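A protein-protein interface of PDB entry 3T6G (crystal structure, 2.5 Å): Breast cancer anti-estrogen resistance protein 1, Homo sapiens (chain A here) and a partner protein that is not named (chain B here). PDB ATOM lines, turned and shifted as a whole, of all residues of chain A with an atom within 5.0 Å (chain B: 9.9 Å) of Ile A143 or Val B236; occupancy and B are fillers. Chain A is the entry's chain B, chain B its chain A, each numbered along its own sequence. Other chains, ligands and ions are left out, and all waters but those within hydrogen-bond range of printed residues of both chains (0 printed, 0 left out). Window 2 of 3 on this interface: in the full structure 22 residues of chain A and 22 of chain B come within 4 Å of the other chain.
No residue of chain B comes within 4 Å of Val A142. Printed residues of chain B within 4 Å of Ile A143: Val B236 and Leu B240. No residue of chain B comes within 4 Å of Ser A145. No residue of chain B comes within 4 Å of Ala A146. Of the printed residues of chain B, His A147 touches Leu B243 (3.6 Å). Of the printed residues of chain B, Val A184 touches Glu B237 (3.8 Å) and Leu B240 (3.6 Å). Printed residues of chain A within 4 Å of Leu B216: Leu A144. Of the printed residues of chain A, Gly B235 touches Lys A140 (3.6 Å). Of chain A, only Lys A140 (3.2 Å) and Ile A143 (3.6 Å) come within 4 Å of Val B236. Of the printed residues of chain A, Glu B237 touches Val A184 (3.8 Å). Of the printed residues of chain A, Leu B243 touches His A147. The nearest printed residue of chain B that does not touch Ile A143 is Leu B243 (4.3 Å). The nearest printed residue of chain A that does not touch Gly B235 is Val A136 (6.1 Å).
Lys A140 touches His B234 (CE to O, 3.5 Å). Lys A140 touches Gly B235 (CD to C, 3.6 Å). CD of Lys A140 touches N of Val B236 (3.2 Å). Val B236 touches Ile A143. Ile A143 touches Leu B240. Leu A144 touches Leu B216. Leu B243 touches His A147 (O to CE1, 3.6 Å). CG2 of Val A184 touches CG of Glu B237 (3.8 Å). Val A184 touches Leu B240.
Printed residues of chain A that touch a printed residue of chain B: Lys A140, Ile A143, Leu A144, His A147 and Val A184. Hydrophobic or aromatic side chains of chain A that line the printed part of chain B: Ile A143, Leu A144, His A147 and Val A184. Of the 14 printed residues of chain B, 7 touch a printed residue of chain A. Hydrophobic or aromatic side chains of chain B that line the printed part of chain A: Leu B216, Val B236, Leu B240 and Leu B243. Among the printed residues, 9 pairs touch across the chains.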
ATOM      1  N   VAL A 136     -10.343  28.570   2.842  1.00  0.00           N
ATOM      2  CA  VAL A 136     -11.231  28.549   3.989  1.00  0.00           C
ATOM      3  C   VAL A 136     -12.625  28.975   3.561  1.00  0.00           C
ATOM      4  O   VAL A 136     -13.615  28.373   3.966  1.00  0.00           O
ATOM      5  CB  VAL A 136     -10.750  29.444   5.114  1.00  0.00           C
ATOM      6  CG1 VAL A 136     -11.881  29.654   6.131  1.00  0.00           C
ATOM      7  CG2 VAL A 136      -9.540  28.810   5.759  1.00  0.00           C
ATOM      8  N   SER A 139     -14.144  26.052   1.844  1.00  0.00           N
ATOM      9  CA  SER A 139     -14.625  25.155   2.889  1.00  0.00           C
ATOM     10  C   SER A 139     -16.020  25.532   3.373  1.00  0.00           C
ATOM     11  O   SER A 139     -16.882  24.670   3.504  1.00  0.00           O
ATOM     12  CB  SER A 139     -13.692  25.149   4.088  1.00  0.00           C
ATOM     13  OG  SER A 139     -12.726  24.127   3.947  1.00  0.00           O
ATOM     14  N   LYS A 140     -16.231  26.810   3.672  1.00  0.00           N
ATOM     15  CA  LYS A 140     -17.521  27.245   4.193  1.00  0.00           C
ATOM     16  C   LYS A 140     -18.617  26.868   3.213  1.00  0.00           C
ATOM     17  O   LYS A 140     -19.627  26.276   3.602  1.00  0.00           O
ATOM     18  CB  LYS A 140     -17.545  28.747   4.489  1.00  0.00           C
ATOM     19  CG  LYS A 140     -16.725  29.138   5.716  1.00  0.00           C
ATOM     20  CD  LYS A 140     -17.058  30.562   6.238  1.00  0.00           C
ATOM     21  CE  LYS A 140     -16.609  31.682   5.286  1.00  0.00           C
ATOM     22  NZ  LYS A 140     -15.199  32.177   5.500  1.00  0.00           N
ATOM     23  N   PHE A 141     -18.400  27.182   1.939  1.00  0.00           N
ATOM     24  CA  PHE A 141     -19.362  26.823   0.907  1.00  0.00           C
ATOM     25  C   PHE A 141     -19.620  25.297   0.873  1.00  0.00           C
ATOM     26  O   PHE A 141     -20.765  24.861   0.772  1.00  0.00           O
ATOM     27  CB  PHE A 141     -18.902  27.333  -0.458  1.00  0.00           C
ATOM     28  CG  PHE A 141     -19.946  27.211  -1.534  1.00  0.00           C
ATOM     29  CD1 PHE A 141     -21.299  27.319  -1.227  1.00  0.00           C
ATOM     30  CD2 PHE A 141     -19.580  26.983  -2.857  1.00  0.00           C
ATOM     31  CE1 PHE A 141     -22.268  27.208  -2.215  1.00  0.00           C
ATOM     32  CE2 PHE A 141     -20.549  26.869  -3.851  1.00  0.00           C
ATOM     33  CZ  PHE A 141     -21.895  26.984  -3.525  1.00  0.00           C
ATOM     34  N   VAL A 142     -18.561  24.491   0.971  1.00  0.00           N
ATOM     35  CA  VAL A 142     -18.715  23.043   0.971  1.00  0.00           C
ATOM     36  C   VAL A 142     -19.518  22.547   2.173  1.00  0.00           C
ATOM     37  O   VAL A 142     -20.341  21.656   2.042  1.00  0.00           O
ATOM     38  CB  VAL A 142     -17.347  22.310   0.879  1.00  0.00           C
ATOM     39  CG1 VAL A 142     -17.459  20.858   1.323  1.00  0.00           C
ATOM     40  CG2 VAL A 142     -16.803  22.387  -0.539  1.00  0.00           C
ATOM     41  N   ILE A 143     -19.275  23.129   3.337  1.00  0.00           N
ATOM     42  CA  ILE A 143     -19.944  22.738   4.573  1.00  0.00           C
ATOM     43  C   ILE A 143     -21.412  23.161   4.546  1.00  0.00           C
ATOM     44  O   ILE A 143     -22.305  22.453   5.045  1.00  0.00           O
ATOM     45  CB  ILE A 143     -19.248  23.403   5.769  1.00  0.00           C
ATOM     46  CG1 ILE A 143     -17.894  22.742   6.014  1.00  0.00           C
ATOM     47  CG2 ILE A 143     -20.092  23.313   7.017  1.00  0.00           C
ATOM     48  CD1 ILE A 143     -16.972  23.554   6.890  1.00  0.00           C
ATOM     49  N   LEU A 144     -21.655  24.323   3.953  1.00  0.00           N
ATOM     50  CA  LEU A 144     -23.003  24.845   3.810  1.00  0.00           C
ATOM     51  C   LEU A 144     -23.870  23.889   2.982  1.00  0.00           C
ATOM     52  O   LEU A 144     -24.910  23.422   3.454  1.00  0.00           O
ATOM     53  CB  LEU A 144     -22.947  26.214   3.137  1.00  0.00           C
ATOM     54  CG  LEU A 144     -24.085  27.217   3.329  1.00  0.00           C
ATOM     55  CD1 LEU A 144     -25.050  26.817   4.451  1.00  0.00           C
ATOM     56  CD2 LEU A 144     -23.487  28.583   3.607  1.00  0.00           C
ATOM     57  N   SER A 145     -23.436  23.599   1.751  1.00  0.00           N
ATOM     58  CA  SER A 145     -24.230  22.801   0.814  1.00  0.00           C
ATOM     59  C   SER A 145     -24.516  21.437   1.388  1.00  0.00           C
ATOM     60  O   SER A 145     -25.613  20.913   1.242  1.00  0.00           O
ATOM     61  CB  SER A 145     -23.511  22.624  -0.523  1.00  0.00           C
ATOM     62  OG  SER A 145     -23.050  23.864  -1.013  1.00  0.00           O
ATOM     63  N   ALA A 146     -23.519  20.873   2.052  1.00  0.00           N
ATOM     64  CA  ALA A 146     -23.613  19.507   2.526  1.00  0.00           C
ATOM     65  C   ALA A 146     -24.515  19.456   3.725  1.00  0.00           C
ATOM     66  O   ALA A 146     -25.154  18.433   3.953  1.00  0.00           O
ATOM     67  CB  ALA A 146     -22.226  18.938   2.885  1.00  0.00           C
ATOM     68  N   HIS A 147     -24.551  20.544   4.502  1.00  0.00           N
ATOM     69  CA  HIS A 147     -25.445  20.593   5.663  1.00  0.00           C
ATOM     70  C   HIS A 147     -26.927  20.561   5.263  1.00  0.00           C
ATOM     71  O   HIS A 147     -27.760  20.066   6.009  1.00  0.00           O
ATOM     72  CB  HIS A 147     -25.150  21.754   6.617  1.00  0.00           C
ATOM     73  CG  HIS A 147     -25.452  21.416   8.042  1.00  0.00           C
ATOM     74  ND1 HIS A 147     -26.738  21.382   8.544  1.00  0.00           N
ATOM     75  CD2 HIS A 147     -24.642  21.034   9.057  1.00  0.00           C
ATOM     76  CE1 HIS A 147     -26.702  21.003   9.810  1.00  0.00           C
ATOM     77  NE2 HIS A 147     -25.444  20.783  10.147  1.00  0.00           N
ATOM     78  N   LEU A 180     -18.486  16.974   8.834  1.00  0.00           N
ATOM     79  CA  LEU A 180     -18.478  18.407   8.622  1.00  0.00           C
ATOM     80  C   LEU A 180     -17.641  19.066   9.720  1.00  0.00           C
ATOM     81  O   LEU A 180     -16.891  19.995   9.463  1.00  0.00           O
ATOM     82  CB  LEU A 180     -19.883  18.949   8.551  1.00  0.00           C
ATOM     83  CG  LEU A 180     -20.665  18.582   7.292  1.00  0.00           C
ATOM     84  CD1 LEU A 180     -21.967  19.356   7.290  1.00  0.00           C
ATOM     85  CD2 LEU A 180     -19.828  18.948   6.087  1.00  0.00           C
ATOM     86  N   ILE A 183     -14.112  18.436   8.716  1.00  0.00           N
ATOM     87  CA  ILE A 183     -13.727  19.402   7.710  1.00  0.00           C
ATOM     88  C   ILE A 183     -13.319  20.729   8.358  1.00  0.00           C
ATOM     89  O   ILE A 183     -12.261  21.270   8.025  1.00  0.00           O
ATOM     90  CB  ILE A 183     -14.831  19.570   6.665  1.00  0.00           C
ATOM     91  CG1 ILE A 183     -14.880  18.304   5.803  1.00  0.00           C
ATOM     92  CG2 ILE A 183     -14.604  20.794   5.790  1.00  0.00           C
ATOM     93  CD1 ILE A 183     -16.191  18.100   5.141  1.00  0.00           C
ATOM     94  N   VAL A 184     -14.137  21.234   9.287  1.00  0.00           N
ATOM     95  CA  VAL A 184     -13.799  22.456  10.002  1.00  0.00           C
ATOM     96  C   VAL A 184     -12.493  22.293  10.777  1.00  0.00           C
ATOM     97  O   VAL A 184     -11.625  23.149  10.699  1.00  0.00           O
ATOM     98  CB  VAL A 184     -14.908  22.952  10.980  1.00  0.00           C
ATOM     99  CG1 VAL A 184     -15.318  21.849  11.910  1.00  0.00           C
ATOM    100  CG2 VAL A 184     -14.361  24.115  11.830  1.00  0.00           C
ATOM    101  N   LEU B 215     -27.685  32.818   5.931  1.00  0.00           N
ATOM    102  CA  LEU B 215     -26.794  31.839   5.346  1.00  0.00           C
ATOM    103  C   LEU B 215     -27.485  31.130   4.170  1.00  0.00           C
ATOM    104  O   LEU B 215     -27.123  31.339   3.010  1.00  0.00           O
ATOM    105  CB  LEU B 215     -26.389  30.821   6.410  1.00  0.00           C
ATOM    106  CG  LEU B 215     -25.008  30.951   7.051  1.00  0.00           C
ATOM    107  CD1 LEU B 215     -24.465  32.319   6.831  1.00  0.00           C
ATOM    108  CD2 LEU B 215     -25.044  30.619   8.531  1.00  0.00           C
ATOM    109  N   LEU B 216     -28.496  30.315   4.464  1.00  0.00           N
ATOM    110  CA  LEU B 216     -29.115  29.481   3.437  1.00  0.00           C
ATOM    111  C   LEU B 216     -29.633  30.260   2.238  1.00  0.00           C
ATOM    112  O   LEU B 216     -30.026  29.667   1.240  1.00  0.00           O
ATOM    113  CB  LEU B 216     -30.254  28.647   4.000  1.00  0.00           C
ATOM    114  CG  LEU B 216     -30.148  28.024   5.393  1.00  0.00           C
ATOM    115  CD1 LEU B 216     -31.252  26.976   5.589  1.00  0.00           C
ATOM    116  CD2 LEU B 216     -28.794  27.420   5.608  1.00  0.00           C
ATOM    117  N   GLU B 233     -19.512  36.513   5.355  1.00  0.00           N
ATOM    118  CA  GLU B 233     -19.570  37.345   6.556  1.00  0.00           C
ATOM    119  C   GLU B 233     -19.008  36.634   7.794  1.00  0.00           C
ATOM    120  O   GLU B 233     -18.004  37.072   8.364  1.00  0.00           O
ATOM    121  CB  GLU B 233     -21.006  37.814   6.819  1.00  0.00           C
ATOM    122  CG  GLU B 233     -21.128  38.856   7.922  1.00  0.00           C
ATOM    123  CD  GLU B 233     -22.549  39.377   8.084  1.00  0.00           C
ATOM    124  OE1 GLU B 233     -22.839  39.984   9.137  1.00  0.00           O
ATOM    125  OE2 GLU B 233     -23.378  39.186   7.163  1.00  0.00           O
ATOM    126  N   HIS B 234     -19.667  35.551   8.206  1.00  0.00           N
ATOM    127  CA  HIS B 234     -19.225  34.742   9.342  1.00  0.00           C
ATOM    128  C   HIS B 234     -17.981  33.923   9.002  1.00  0.00           C
ATOM    129  O   HIS B 234     -17.586  33.801   7.838  1.00  0.00           O
ATOM    130  CB  HIS B 234     -20.323  33.768   9.789  1.00  0.00           C
ATOM    131  CG  HIS B 234     -21.555  34.427  10.328  1.00  0.00           C
ATOM    132  ND1 HIS B 234     -21.595  35.042  11.562  1.00  0.00           N
ATOM    133  CD2 HIS B 234     -22.802  34.544   9.809  1.00  0.00           C
ATOM    134  CE1 HIS B 234     -22.811  35.519  11.772  1.00  0.00           C
ATOM    135  NE2 HIS B 234     -23.561  35.231  10.725  1.00  0.00           N
ATOM    136  N   GLY B 235     -17.377  33.339  10.028  1.00  0.00           N
ATOM    137  CA  GLY B 235     -16.206  32.525   9.825  1.00  0.00           C
ATOM    138  C   GLY B 235     -16.587  31.060   9.818  1.00  0.00           C
ATOM    139  O   GLY B 235     -17.594  30.702  10.410  1.00  0.00           O
ATOM    140  N   VAL B 236     -15.771  30.212   9.191  1.00  0.00           N
ATOM    141  CA  VAL B 236     -16.113  28.806   9.077  1.00  0.00           C
ATOM    142  C   VAL B 236     -16.579  28.167  10.389  1.00  0.00           C
ATOM    143  O   VAL B 236     -17.331  27.206  10.373  1.00  0.00           O
ATOM    144  CB  VAL B 236     -14.968  27.965   8.469  1.00  0.00           C
ATOM    145  CG1 VAL B 236     -13.937  27.589   9.525  1.00  0.00           C
ATOM    146  CG2 VAL B 236     -15.536  26.718   7.863  1.00  0.00           C
ATOM    147  N   GLU B 237     -16.146  28.693  11.526  1.00  0.00           N
ATOM    148  CA  GLU B 237     -16.500  28.065  12.798  1.00  0.00           C
ATOM    149  C   GLU B 237     -17.891  28.441  13.343  1.00  0.00           C
ATOM    150  O   GLU B 237     -18.594  27.587  13.897  1.00  0.00           O
ATOM    151  CB  GLU B 237     -15.424  28.322  13.849  1.00  0.00           C
ATOM    152  CG  GLU B 237     -14.379  27.239  13.941  1.00  0.00           C
ATOM    153  CD  GLU B 237     -13.287  27.612  14.896  1.00  0.00           C
ATOM    154  OE1 GLU B 237     -12.946  26.801  15.785  1.00  0.00           O
ATOM    155  OE2 GLU B 237     -12.775  28.739  14.758  1.00  0.00           O
ATOM    156  N   VAL B 238     -18.293  29.700  13.197  1.00  0.00           N
ATOM    157  CA  VAL B 238     -19.626  30.067  13.647  1.00  0.00           C
ATOM    158  C   VAL B 238     -20.659  29.612  12.633  1.00  0.00           C
ATOM    159  O   VAL B 238     -21.769  29.215  13.001  1.00  0.00           O
ATOM    160  CB  VAL B 238     -19.809  31.585  13.929  1.00  0.00           C
ATOM    161  CG1 VAL B 238     -18.659  32.109  14.750  1.00  0.00           C
ATOM    162  CG2 VAL B 238     -19.990  32.369  12.634  1.00  0.00           C
ATOM    163  N   VAL B 239     -20.297  29.687  11.358  1.00  0.00           N
ATOM    164  CA  VAL B 239     -21.136  29.130  10.314  1.00  0.00           C
ATOM    165  C   VAL B 239     -21.556  27.712  10.699  1.00  0.00           C
ATOM    166  O   VAL B 239     -22.728  27.393  10.664  1.00  0.00           O
ATOM    167  CB  VAL B 239     -20.439  29.145   8.943  1.00  0.00           C
ATOM    168  CG1 VAL B 239     -21.045  28.079   8.001  1.00  0.00           C
ATOM    169  CG2 VAL B 239     -20.528  30.538   8.342  1.00  0.00           C
ATOM    170  N   LEU B 240     -20.622  26.869  11.108  1.00  0.00           N
ATOM    171  CA  LEU B 240     -21.028  25.527  11.514  1.00  0.00           C
ATOM    172  C   LEU B 240     -21.795  25.558  12.844  1.00  0.00           C
ATOM    173  O   LEU B 240     -22.520  24.638  13.192  1.00  0.00           O
ATOM    174  CB  LEU B 240     -19.828  24.575  11.589  1.00  0.00           C
ATOM    175  CG  LEU B 240     -20.117  23.094  11.909  1.00  0.00           C
ATOM    176  CD1 LEU B 240     -20.912  22.393  10.813  1.00  0.00           C
ATOM    177  CD2 LEU B 240     -18.829  22.333  12.186  1.00  0.00           C
ATOM    178  N   ALA B 241     -21.632  26.635  13.586  1.00  0.00           N
ATOM    179  CA  ALA B 241     -22.268  26.748  14.881  1.00  0.00           C
ATOM    180  C   ALA B 241     -23.750  27.077  14.689  1.00  0.00           C
ATOM    181  O   ALA B 241     -24.623  26.504  15.339  1.00  0.00           O
ATOM    182  CB  ALA B 241     -21.573  27.811  15.705  1.00  0.00           C
ATOM    183  N   HIS B 242     -24.042  27.979  13.768  1.00  0.00           N
ATOM    184  CA  HIS B 242     -25.426  28.258  13.460  1.00  0.00           C
ATOM    185  C   HIS B 242     -26.123  27.054  12.870  1.00  0.00           C
ATOM    186  O   HIS B 242     -27.277  26.796  13.206  1.00  0.00           O
ATOM    187  CB  HIS B 242     -25.547  29.484  12.568  1.00  0.00           C
ATOM    188  CG  HIS B 242     -25.208  30.759  13.282  1.00  0.00           C
ATOM    189  ND1 HIS B 242     -24.635  31.848  12.651  1.00  0.00           N
ATOM    190  CD2 HIS B 242     -25.345  31.106  14.583  1.00  0.00           C
ATOM    191  CE1 HIS B 242     -24.440  32.812  13.532  1.00  0.00           C
ATOM    192  NE2 HIS B 242     -24.852  32.385  14.712  1.00  0.00           N
ATOM    193  N   LEU B 243     -25.421  26.295  12.027  1.00  0.00           N
ATOM    194  CA  LEU B 243     -26.033  25.139  11.373  1.00  0.00           C
ATOM    195  C   LEU B 243     -26.317  24.009  12.355  1.00  0.00           C
ATOM    196  O   LEU B 243     -27.383  23.411  12.329  1.00  0.00           O
ATOM    197  CB  LEU B 243     -25.175  24.624  10.227  1.00  0.00           C
ATOM    198  CG  LEU B 243     -25.054  25.523   9.004  1.00  0.00           C
ATOM    199  CD1 LEU B 243     -23.921  24.996   8.098  1.00  0.00           C
ATOM    200  CD2 LEU B 243     -26.368  25.598   8.248  1.00  0.00           C
ATOM    201  N   GLU B 244     -25.375  23.715  13.231  1.00  0.00           N
ATOM    202  CA  GLU B 244     -25.627  22.649  14.190  1.00  0.00           C
ATOM    203  C   GLU B 244     -26.764  23.050  15.116  1.00  0.00           C
ATOM    204  O   GLU B 244     -27.616  22.238  15.454  1.00  0.00           O
ATOM    205  CB  GLU B 244     -24.371  22.308  14.993  1.00  0.00           C
ATOM    206  CG  GLU B 244     -23.379  21.421  14.239  1.00  0.00           C
ATOM    207  CD  GLU B 244     -22.160  21.084  15.074  1.00  0.00           C
ATOM    208  OE1 GLU B 244     -21.451  22.013  15.514  1.00  0.00           O
ATOM    209  OE2 GLU B 244     -21.915  19.893  15.315  1.00  0.00           O
